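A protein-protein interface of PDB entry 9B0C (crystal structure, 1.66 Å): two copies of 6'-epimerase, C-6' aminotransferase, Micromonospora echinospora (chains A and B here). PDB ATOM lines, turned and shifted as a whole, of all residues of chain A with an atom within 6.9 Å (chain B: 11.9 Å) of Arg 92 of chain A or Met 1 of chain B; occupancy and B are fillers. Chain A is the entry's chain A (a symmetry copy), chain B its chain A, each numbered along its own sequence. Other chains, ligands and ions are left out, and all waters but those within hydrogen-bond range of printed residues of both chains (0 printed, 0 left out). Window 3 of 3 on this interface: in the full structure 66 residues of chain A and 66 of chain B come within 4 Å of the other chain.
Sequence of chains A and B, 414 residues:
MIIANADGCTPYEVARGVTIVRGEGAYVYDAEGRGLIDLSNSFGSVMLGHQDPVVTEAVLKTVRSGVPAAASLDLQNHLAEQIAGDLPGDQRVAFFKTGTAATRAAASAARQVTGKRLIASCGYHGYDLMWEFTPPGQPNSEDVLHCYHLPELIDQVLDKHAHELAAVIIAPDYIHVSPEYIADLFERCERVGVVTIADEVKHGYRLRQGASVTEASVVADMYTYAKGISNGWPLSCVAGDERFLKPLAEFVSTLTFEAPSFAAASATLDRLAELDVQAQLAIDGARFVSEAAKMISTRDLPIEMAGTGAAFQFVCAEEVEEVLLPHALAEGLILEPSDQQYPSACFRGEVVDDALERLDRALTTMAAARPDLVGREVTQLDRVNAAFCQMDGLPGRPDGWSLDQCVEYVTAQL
No position is printed for both chains.
Of the 14 pairs that touch across the chains among the printed residues, none has its exchanged pair printed and touching as well.
Printed residues of chain B that touch a printed residue of chain A: Met 1, Ile 2, Ile 3, Ala 4 and Asn 5.
Hydrophobic or aromatic side chains of chain B that line the printed part of chain A: Ile 2, Ile 3 and Ala 4.
Along chain B the printed residues that touch a printed residue of chain A span positions 1 to 5.
The side-chain amide oxygen (OE1) of Gln 91 of chain A lies close to the backbone carbonyl oxygen (O) of Ala 84 of chain A.
The side-chain amide oxygen of Gln 91 of chain A sits close to the backbone carbonyl oxygen of Leu 87 of chain A (3.5 Å).
The side-chain carboxylate (OD1) of Asp 90 of chain A is in salt-bridge range of the guanidinium group (NH2) of Arg 92 of chain A.
N of Arg 92 of chain A is in hydrogen-bond range of O of Gly 240 of chain A, 2.9 Å away.
The guanidinium group (NH2) of Arg 92 of chain A lies within salt-bridge range of the side-chain carboxylate (OE2) of Glu 242 of chain A, at 3.7 Å.
The backbone NH (N) of Ala 94 of chain A lies within hydrogen-bond range of the backbone carbonyl oxygen (O) of Val 238 of chain A (2.9 Å).
Printed residues of chain B within 4 Å of Asn 77 of chain A: Ile 2 (2.9 Å) and Ile 3 (3.5 Å).
Ala 84 of chain A touches one residue of chain B.
No residue of chain B comes within 4 Å of Asp 90 of chain A.
Arg 92 of chain A touches just these residues of chain B: Met 1 and Ile 2.
Ala 94 of chain A touches one residue of chain B.
No residue of chain B comes within 4 Å of Gly 240 of chain A.
No residue of chain B comes within 4 Å of Glu 242 of chain A.
Of the printed residues of chain A, Met 1 of chain B touches Arg 92.
Of the printed residues of chain A, Ala 4 of chain B touches Val 93 (2.7 Å) and Leu 245 (3.6 Å).
Printed residues of chain A within 4 Å of Asn 5 of chain B: Ala 94 (3.4 Å).
Arg 16 of chain B touches none of the printed residues of chain A.
The nearest residue of chain A that does not touch Met 1 of chain B is Asn 77 of chain A (4.4 Å).
OD1 of Asn 77 of chain A touches CG2 of Ile 2 of chain B, at 2.9 Å.
N of Asn 77 of chain A touches CD1 of Ile 3 of chain B, at 3.5 Å.
Ile 2 of chain B touches Ala 80 of chain A.
CG1 of Ile 3 of chain B touches CB of Ala 80 of chain A, 3.7 Å away.
Glu 81 of chain A touches Ile 2 of chain B.
Ile 2 of chain B touches Ala 84 of chain A.
CG1 of Ile 2 of chain B touches O of Gln 91 of chain A (3.6 Å).
Ile 2 of chain B touches Arg 92 of chain A.
O of Val 93 of chain A touches CA of Ile 3 of chain B, at 3.3 Å.
CB of Ala 4 of chain B touches O of Leu 245 of chain A (3.6 Å).
The backbone carbonyl oxygen of Ile 2 of chain B sits at hydrogen-bond distance from the backbone NH of Val 93 of chain A (2.9 Å).
N of Ala 4 of chain B is in hydrogen-bond range of O of Val 93 of chain A (2.7 Å).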
ATOM      1  N   ASN A  77      -6.535   6.991 -32.383  1.00  0.00           N
ATOM      2  CA  ASN A  77      -6.544   7.443 -30.995  1.00  0.00           C
ATOM      3  C   ASN A  77      -7.969   7.531 -30.459  1.00  0.00           C
ATOM      4  O   ASN A  77      -8.226   7.204 -29.295  1.00  0.00           O
ATOM      5  CB  ASN A  77      -5.862   8.806 -30.885  1.00  0.00           C
ATOM      6  CG  ASN A  77      -5.594   9.201 -29.455  1.00  0.00           C
ATOM      7  OD1 ASN A  77      -4.966   8.451 -28.710  1.00  0.00           O
ATOM      8  ND2 ASN A  77      -6.100  10.356 -29.047  1.00  0.00           N
ATOM      9  N   ALA A  80      -9.138   4.163 -29.385  1.00  0.00           N
ATOM     10  CA  ALA A  80      -8.530   3.772 -28.122  1.00  0.00           C
ATOM     11  C   ALA A  80      -9.208   4.474 -26.952  1.00  0.00           C
ATOM     12  O   ALA A  80      -9.451   3.857 -25.909  1.00  0.00           O
ATOM     13  CB  ALA A  80      -7.027   4.078 -28.128  1.00  0.00           C
ATOM     14  N   GLU A  81      -9.534   5.763 -27.110  1.00  0.00           N
ATOM     15  CA  GLU A  81     -10.277   6.465 -26.058  1.00  0.00           C
ATOM     16  C   GLU A  81     -11.655   5.854 -25.819  1.00  0.00           C
ATOM     17  O   GLU A  81     -12.107   5.760 -24.672  1.00  0.00           O
ATOM     18  CB  GLU A  81     -10.422   7.951 -26.401  1.00  0.00           C
ATOM     19  CG  GLU A  81      -9.086   8.665 -26.433  1.00  0.00           C
ATOM     20  CD  GLU A  81      -9.200  10.114 -26.873  1.00  0.00           C
ATOM     21  OE1 GLU A  81     -10.221  10.485 -27.498  1.00  0.00           O
ATOM     22  OE2 GLU A  81      -8.258  10.883 -26.575  1.00  0.00           O
ATOM     23  N   ILE A  83     -12.566   2.743 -26.194  1.00  0.00           N
ATOM     24  CA  ILE A  83     -12.398   1.484 -25.472  1.00  0.00           C
ATOM     25  C   ILE A  83     -11.956   1.742 -24.037  1.00  0.00           C
ATOM     26  O   ILE A  83     -12.484   1.156 -23.082  1.00  0.00           O
ATOM     27  CB  ILE A  83     -11.389   0.590 -26.220  1.00  0.00           C
ATOM     28  CG1 ILE A  83     -11.991   0.121 -27.545  1.00  0.00           C
ATOM     29  CG2 ILE A  83     -10.958  -0.596 -25.349  1.00  0.00           C
ATOM     30  CD1 ILE A  83     -10.938  -0.375 -28.542  1.00  0.00           C
ATOM     31  N   ALA A  84     -10.952   2.598 -23.856  1.00  0.00           N
ATOM     32  CA  ALA A  84     -10.465   2.819 -22.502  1.00  0.00           C
ATOM     33  C   ALA A  84     -11.520   3.464 -21.624  1.00  0.00           C
ATOM     34  O   ALA A  84     -11.579   3.179 -20.426  1.00  0.00           O
ATOM     35  CB  ALA A  84      -9.195   3.667 -22.524  1.00  0.00           C
ATOM     36  N   LEU A  87     -13.783   1.191 -19.494  1.00  0.00           N
ATOM     37  CA  LEU A  87     -13.225   0.347 -18.450  1.00  0.00           C
ATOM     38  C   LEU A  87     -12.907   1.183 -17.221  1.00  0.00           C
ATOM     39  O   LEU A  87     -12.516   2.345 -17.351  1.00  0.00           O
ATOM     40  CB  LEU A  87     -11.947  -0.334 -18.930  1.00  0.00           C
ATOM     41  CG  LEU A  87     -12.205  -1.406 -20.002  1.00  0.00           C
ATOM     42  CD1 LEU A  87     -10.927  -1.699 -20.767  1.00  0.00           C
ATOM     43  CD2 LEU A  87     -12.703  -2.689 -19.307  1.00  0.00           C
ATOM     44  N   ASP A  90      -7.452   3.606 -15.467  1.00  0.00           N
ATOM     45  CA  ASP A  90      -6.683   4.314 -16.485  1.00  0.00           C
ATOM     46  C   ASP A  90      -6.041   3.254 -17.373  1.00  0.00           C
ATOM     47  O   ASP A  90      -5.138   2.538 -16.928  1.00  0.00           O
ATOM     48  CB  ASP A  90      -5.638   5.204 -15.805  1.00  0.00           C
ATOM     49  CG  ASP A  90      -4.960   6.167 -16.760  1.00  0.00           C
ATOM     50  OD1 ASP A  90      -5.072   5.985 -17.985  1.00  0.00           O
ATOM     51  OD2 ASP A  90      -4.301   7.118 -16.271  1.00  0.00           O
ATOM     52  N   GLN A  91      -6.532   3.111 -18.602  1.00  0.00           N
ATOM     53  CA  GLN A  91      -6.006   2.107 -19.518  1.00  0.00           C
ATOM     54  C   GLN A  91      -5.322   2.750 -20.715  1.00  0.00           C
ATOM     55  O   GLN A  91      -5.697   3.834 -21.161  1.00  0.00           O
ATOM     56  CB  GLN A  91      -7.127   1.205 -20.038  1.00  0.00           C
ATOM     57  CG  GLN A  91      -7.548   0.158 -19.034  1.00  0.00           C
ATOM     58  CD  GLN A  91      -8.590   0.727 -18.098  1.00  0.00           C
ATOM     59  OE1 GLN A  91      -9.271   1.706 -18.434  1.00  0.00           O
ATOM     60  NE2 GLN A  91      -8.735   0.117 -16.927  1.00  0.00           N
ATOM     61  N   ARG A  92      -4.326   2.041 -21.234  1.00  0.00           N
ATOM     62  CA  ARG A  92      -3.808   2.211 -22.581  1.00  0.00           C
ATOM     63  C   ARG A  92      -4.293   1.037 -23.418  1.00  0.00           C
ATOM     64  O   ARG A  92      -4.701   0.008 -22.883  1.00  0.00           O
ATOM     65  CB  ARG A  92      -2.279   2.245 -22.576  1.00  0.00           C
ATOM     66  CG  ARG A  92      -1.653   3.267 -21.601  1.00  0.00           C
ATOM     67  CD  ARG A  92      -1.950   4.701 -22.013  1.00  0.00           C
ATOM     68  NE  ARG A  92      -1.559   5.657 -20.977  1.00  0.00           N
ATOM     69  CZ  ARG A  92      -2.285   5.994 -19.919  1.00  0.00           C
ATOM     70  NH1 ARG A  92      -3.519   5.547 -19.753  1.00  0.00           N
ATOM     71  NH2 ARG A  92      -1.763   6.815 -19.014  1.00  0.00           N
ATOM     72  N   VAL A  93      -4.223   1.178 -24.745  1.00  0.00           N
ATOM     73  CA  VAL A  93      -4.794   0.187 -25.649  1.00  0.00           C
ATOM     74  C   VAL A  93      -3.771  -0.138 -26.728  1.00  0.00           C
ATOM     75  O   VAL A  93      -3.216   0.772 -27.353  1.00  0.00           O
ATOM     76  CB  VAL A  93      -6.107   0.690 -26.286  1.00  0.00           C
ATOM     77  CG1 VAL A  93      -6.747  -0.385 -27.183  1.00  0.00           C
ATOM     78  CG2 VAL A  93      -7.079   1.168 -25.205  1.00  0.00           C
ATOM     79  N   ALA A  94      -3.516  -1.427 -26.935  1.00  0.00           N
ATOM     80  CA  ALA A  94      -2.675  -1.914 -28.025  1.00  0.00           C
ATOM     81  C   ALA A  94      -3.533  -2.707 -29.006  1.00  0.00           C
ATOM     82  O   ALA A  94      -4.291  -3.580 -28.592  1.00  0.00           O
ATOM     83  CB  ALA A  94      -1.548  -2.792 -27.487  1.00  0.00           C
ATOM     84  N   VAL A 238      -5.689  -5.291 -26.730  1.00  0.00           N
ATOM     85  CA  VAL A 238      -5.423  -5.460 -25.309  1.00  0.00           C
ATOM     86  C   VAL A 238      -5.622  -4.089 -24.687  1.00  0.00           C
ATOM     87  O   VAL A 238      -5.032  -3.113 -25.164  1.00  0.00           O
ATOM     88  CB  VAL A 238      -3.984  -5.944 -25.055  1.00  0.00           C
ATOM     89  CG1 VAL A 238      -3.706  -6.096 -23.548  1.00  0.00           C
ATOM     90  CG2 VAL A 238      -3.686  -7.272 -25.778  1.00  0.00           C
ATOM     91  N   ALA A 239      -6.447  -4.005 -23.645  1.00  0.00           N
ATOM     92  CA  ALA A 239      -6.641  -2.760 -22.898  1.00  0.00           C
ATOM     93  C   ALA A 239      -6.238  -3.020 -21.456  1.00  0.00           C
ATOM     94  O   ALA A 239      -6.636  -4.031 -20.877  1.00  0.00           O
ATOM     95  CB  ALA A 239      -8.090  -2.265 -22.979  1.00  0.00           C
ATOM     96  N   GLY A 240      -5.424  -2.144 -20.881  1.00  0.00           N
ATOM     97  CA  GLY A 240      -4.981  -2.448 -19.533  1.00  0.00           C
ATOM     98  C   GLY A 240      -4.075  -1.378 -18.969  1.00  0.00           C
ATOM     99  O   GLY A 240      -3.794  -0.357 -19.601  1.00  0.00           O
ATOM    100  N   ASP A 241      -3.619  -1.644 -17.752  1.00  0.00           N
ATOM    101  CA  ASP A 241      -2.850  -0.668 -17.001  1.00  0.00           C
ATOM    102  C   ASP A 241      -1.516  -0.383 -17.702  1.00  0.00           C
ATOM    103  O   ASP A 241      -0.920  -1.255 -18.353  1.00  0.00           O
ATOM    104  CB  ASP A 241      -2.646  -1.189 -15.577  1.00  0.00           C
ATOM    105  CG  ASP A 241      -3.944  -1.156 -14.747  1.00  0.00           C
ATOM    106  OD1 ASP A 241      -3.993  -1.808 -13.678  1.00  0.00           O
ATOM    107  OD2 ASP A 241      -4.935  -0.517 -15.182  1.00  0.00           O
ATOM    108  N   GLU A 242      -1.068   0.870 -17.587  1.00  0.00           N
ATOM    109  CA  GLU A 242       0.118   1.351 -18.300  1.00  0.00           C
ATOM    110  C   GLU A 242       1.322   0.444 -18.104  1.00  0.00           C
ATOM    111  O   GLU A 242       2.096   0.207 -19.036  1.00  0.00           O
ATOM    112  CB  GLU A 242       0.445   2.769 -17.815  1.00  0.00           C
ATOM    113  CG  GLU A 242       1.443   3.530 -18.670  1.00  0.00           C
ATOM    114  CD  GLU A 242       1.692   4.943 -18.143  1.00  0.00           C
ATOM    115  OE1 GLU A 242       2.555   5.651 -18.708  1.00  0.00           O
ATOM    116  OE2 GLU A 242       1.037   5.336 -17.148  1.00  0.00           O
ATOM    117  N   ARG A 243       1.497  -0.065 -16.887  1.00  0.00           N
ATOM    118  CA  ARG A 243       2.638  -0.921 -16.590  1.00  0.00           C
ATOM    119  C   ARG A 243       2.664  -2.163 -17.477  1.00  0.00           C
ATOM    120  O   ARG A 243       3.743  -2.632 -17.858  1.00  0.00           O
ATOM    121  CB  ARG A 243       2.587  -1.313 -15.111  1.00  0.00           C
ATOM    122  CG  ARG A 243       3.487  -2.445 -14.692  1.00  0.00           C
ATOM    123  CD  ARG A 243       3.419  -2.598 -13.175  1.00  0.00           C
ATOM    124  NE  ARG A 243       2.110  -2.191 -12.674  1.00  0.00           N
ATOM    125  CZ  ARG A 243       1.247  -3.012 -12.090  1.00  0.00           C
ATOM    126  NH1 ARG A 243       1.563  -4.268 -11.821  1.00  0.00           N
ATOM    127  NH2 ARG A 243       0.036  -2.562 -11.771  1.00  0.00           N
ATOM    128  N   LEU A 245       0.960  -2.336 -20.532  1.00  0.00           N
ATOM    129  CA  LEU A 245       0.862  -1.993 -21.941  1.00  0.00           C
ATOM    130  C   LEU A 245       2.158  -1.397 -22.483  1.00  0.00           C
ATOM    131  O   LEU A 245       2.407  -1.488 -23.687  1.00  0.00           O
ATOM    132  CB  LEU A 245      -0.323  -1.040 -22.151  1.00  0.00           C
ATOM    133  CG  LEU A 245      -1.673  -1.753 -22.397  1.00  0.00           C
ATOM    134  CD1 LEU A 245      -1.786  -2.236 -23.833  1.00  0.00           C
ATOM    135  CD2 LEU A 245      -1.918  -2.953 -21.436  1.00  0.00           C
ATOM    136  N   LYS A 246       3.013  -0.840 -21.621  1.00  0.00           N
ATOM    137  CA  LYS A 246       4.315  -0.350 -22.078  1.00  0.00           C
ATOM    138  C   LYS A 246       5.161  -1.430 -22.761  1.00  0.00           C
ATOM    139  O   LYS A 246       5.776  -1.125 -23.802  1.00  0.00           O
ATOM    140  CB  LYS A 246       5.072   0.271 -20.889  1.00  0.00           C
ATOM    141  CG  LYS A 246       6.495   0.769 -21.197  1.00  0.00           C
ATOM    142  CD  LYS A 246       6.506   1.764 -22.369  1.00  0.00           C
ATOM    143  CE  LYS A 246       7.831   1.770 -23.150  1.00  0.00           C
ATOM    144  NZ  LYS A 246       8.140   0.466 -23.817  1.00  0.00           N
ATOM    145  N   MET B   1      -0.764   8.914 -27.507  1.00  0.00           N
ATOM    146  CA  MET B   1      -1.032   9.127 -26.091  1.00  0.00           C
ATOM    147  C   MET B   1      -1.551   7.847 -25.428  1.00  0.00           C
ATOM    148  O   MET B   1      -0.871   7.246 -24.596  1.00  0.00           O
ATOM    149  CB  MET B   1      -2.034  10.274 -25.912  1.00  0.00           C
ATOM    150  CG  MET B   1      -2.530  10.469 -24.487  1.00  0.00           C
ATOM    151  SD  MET B   1      -4.115  11.336 -24.426  1.00  0.00           S
ATOM    152  CE  MET B   1      -4.307  11.580 -22.659  1.00  0.00           C
ATOM    153  N   ILE B   2      -2.750   7.419 -25.816  1.00  0.00           N
ATOM    154  CA  ILE B   2      -3.399   6.290 -25.162  1.00  0.00           C
ATOM    155  C   ILE B   2      -3.217   4.987 -25.950  1.00  0.00           C
ATOM    156  O   ILE B   2      -3.417   3.897 -25.383  1.00  0.00           O
ATOM    157  CB  ILE B   2      -4.887   6.635 -24.940  1.00  0.00           C
ATOM    158  CG1 ILE B   2      -5.700   5.494 -24.369  1.00  0.00           C
ATOM    159  CG2 ILE B   2      -5.534   6.999 -26.242  1.00  0.00           C
ATOM    160  CD1 ILE B   2      -7.060   5.964 -23.992  1.00  0.00           C
ATOM    161  N   ILE B   3      -2.798   5.061 -27.213  1.00  0.00           N
ATOM    162  CA  ILE B   3      -2.440   3.870 -27.982  1.00  0.00           C
ATOM    163  C   ILE B   3      -1.045   3.418 -27.591  1.00  0.00           C
ATOM    164  O   ILE B   3      -0.057   4.119 -27.837  1.00  0.00           O
ATOM    165  CB  ILE B   3      -2.506   4.122 -29.491  1.00  0.00           C
ATOM    166  CG1 ILE B   3      -3.866   4.633 -29.918  1.00  0.00           C
ATOM    167  CG2 ILE B   3      -2.162   2.832 -30.250  1.00  0.00           C
ATOM    168  CD1 ILE B   3      -3.928   4.813 -31.417  1.00  0.00           C
ATOM    169  N   ALA B   4      -0.954   2.214 -27.039  1.00  0.00           N
ATOM    170  CA  ALA B   4       0.322   1.714 -26.556  1.00  0.00           C
ATOM    171  C   ALA B   4       1.273   1.379 -27.697  1.00  0.00           C
ATOM    172  O   ALA B   4       2.486   1.564 -27.557  1.00  0.00           O
ATOM    173  CB  ALA B   4       0.090   0.489 -25.668  1.00  0.00           C
ATOM    174  N   ASN B   5       0.761   0.885 -28.826  1.00  0.00           N
ATOM    175  CA  ASN B   5       1.677   0.389 -29.847  1.00  0.00           C
ATOM    176  C   ASN B   5       1.621   1.223 -31.125  1.00  0.00           C
ATOM    177  O   ASN B   5       1.536   0.683 -32.231  1.00  0.00           O
ATOM    178  CB  ASN B   5       1.412  -1.102 -30.129  1.00  0.00           C
ATOM    179  CG  ASN B   5       0.015  -1.388 -30.688  1.00  0.00           C
ATOM    180  OD1 ASN B   5      -0.912  -0.585 -30.559  1.00  0.00           O
ATOM    181  ND2 ASN B   5      -0.142  -2.573 -31.275  1.00  0.00           N
ATOM    182  N   ALA B   6       1.690   2.548 -30.991  1.00  0.00           N
ATOM    183  CA  ALA B   6       1.803   3.418 -32.158  1.00  0.00           C
ATOM    184  C   ALA B   6       3.125   4.176 -32.182  1.00  0.00           C
ATOM    185  O   ALA B   6       3.217   5.226 -32.826  1.00  0.00           O
ATOM    186  CB  ALA B   6       0.627   4.394 -32.221  1.00  0.00           C
ATOM    187  N   ASP B   7       4.153   3.665 -31.498  1.00  0.00           N
ATOM    188  CA  ASP B   7       5.447   4.337 -31.409  1.00  0.00           C
ATOM    189  C   ASP B   7       6.188   4.324 -32.743  1.00  0.00           C
ATOM    190  O   ASP B   7       5.711   4.876 -33.741  1.00  0.00           O
ATOM    191  CB  ASP B   7       6.320   3.676 -30.336  1.00  0.00           C
ATOM    192  CG  ASP B   7       6.024   4.190 -28.937  1.00  0.00           C
ATOM    193  OD1 ASP B   7       5.032   4.932 -28.766  1.00  0.00           O
ATOM    194  OD2 ASP B   7       6.791   3.853 -28.007  1.00  0.00           O
ATOM    195  N   GLY B   8       7.365   3.708 -32.763  1.00  0.00           N
ATOM    196  CA  GLY B   8       8.081   3.478 -33.998  1.00  0.00           C
ATOM    197  C   GLY B   8       7.475   2.321 -34.764  1.00  0.00           C
ATOM    198  O   GLY B   8       6.340   1.899 -34.520  1.00  0.00           O
ATOM    199  N   THR B  10       6.056   2.087 -37.374  1.00  0.00           N
ATOM    200  CA  THR B  10       4.944   2.477 -38.223  1.00  0.00           C
ATOM    201  C   THR B  10       5.476   3.205 -39.454  1.00  0.00           C
ATOM    202  O   THR B  10       6.502   3.885 -39.380  1.00  0.00           O
ATOM    203  CB  THR B  10       3.970   3.392 -37.470  1.00  0.00           C
ATOM    204  OG1 THR B  10       4.707   4.343 -36.687  1.00  0.00           O
ATOM    205  CG2 THR B  10       3.081   2.572 -36.535  1.00  0.00           C
ATOM    206  N   ARG B  16       5.356  12.832 -40.008  1.00  0.00           N
ATOM    207  CA  ARG B  16       4.624  13.022 -38.756  1.00  0.00           C
ATOM    208  C   ARG B  16       4.362  14.490 -38.429  1.00  0.00           C
ATOM    209  O   ARG B  16       3.577  14.774 -37.515  1.00  0.00           O
ATOM    210  CB  ARG B  16       5.382  12.366 -37.597  1.00  0.00           C
ATOM    211  CG  ARG B  16       4.918  10.950 -37.223  1.00  0.00           C
ATOM    212  CD  ARG B  16       3.427  10.869 -36.887  1.00  0.00           C
ATOM    213  NE  ARG B  16       2.604  10.349 -37.978  1.00  0.00           N
ATOM    214  CZ  ARG B  16       2.476   9.060 -38.280  1.00  0.00           C
ATOM    215  NH1 ARG B  16       3.153   8.125 -37.632  1.00  0.00           N
ATOM    216  NH2 ARG B  16       1.648   8.700 -39.258  1.00  0.00           N
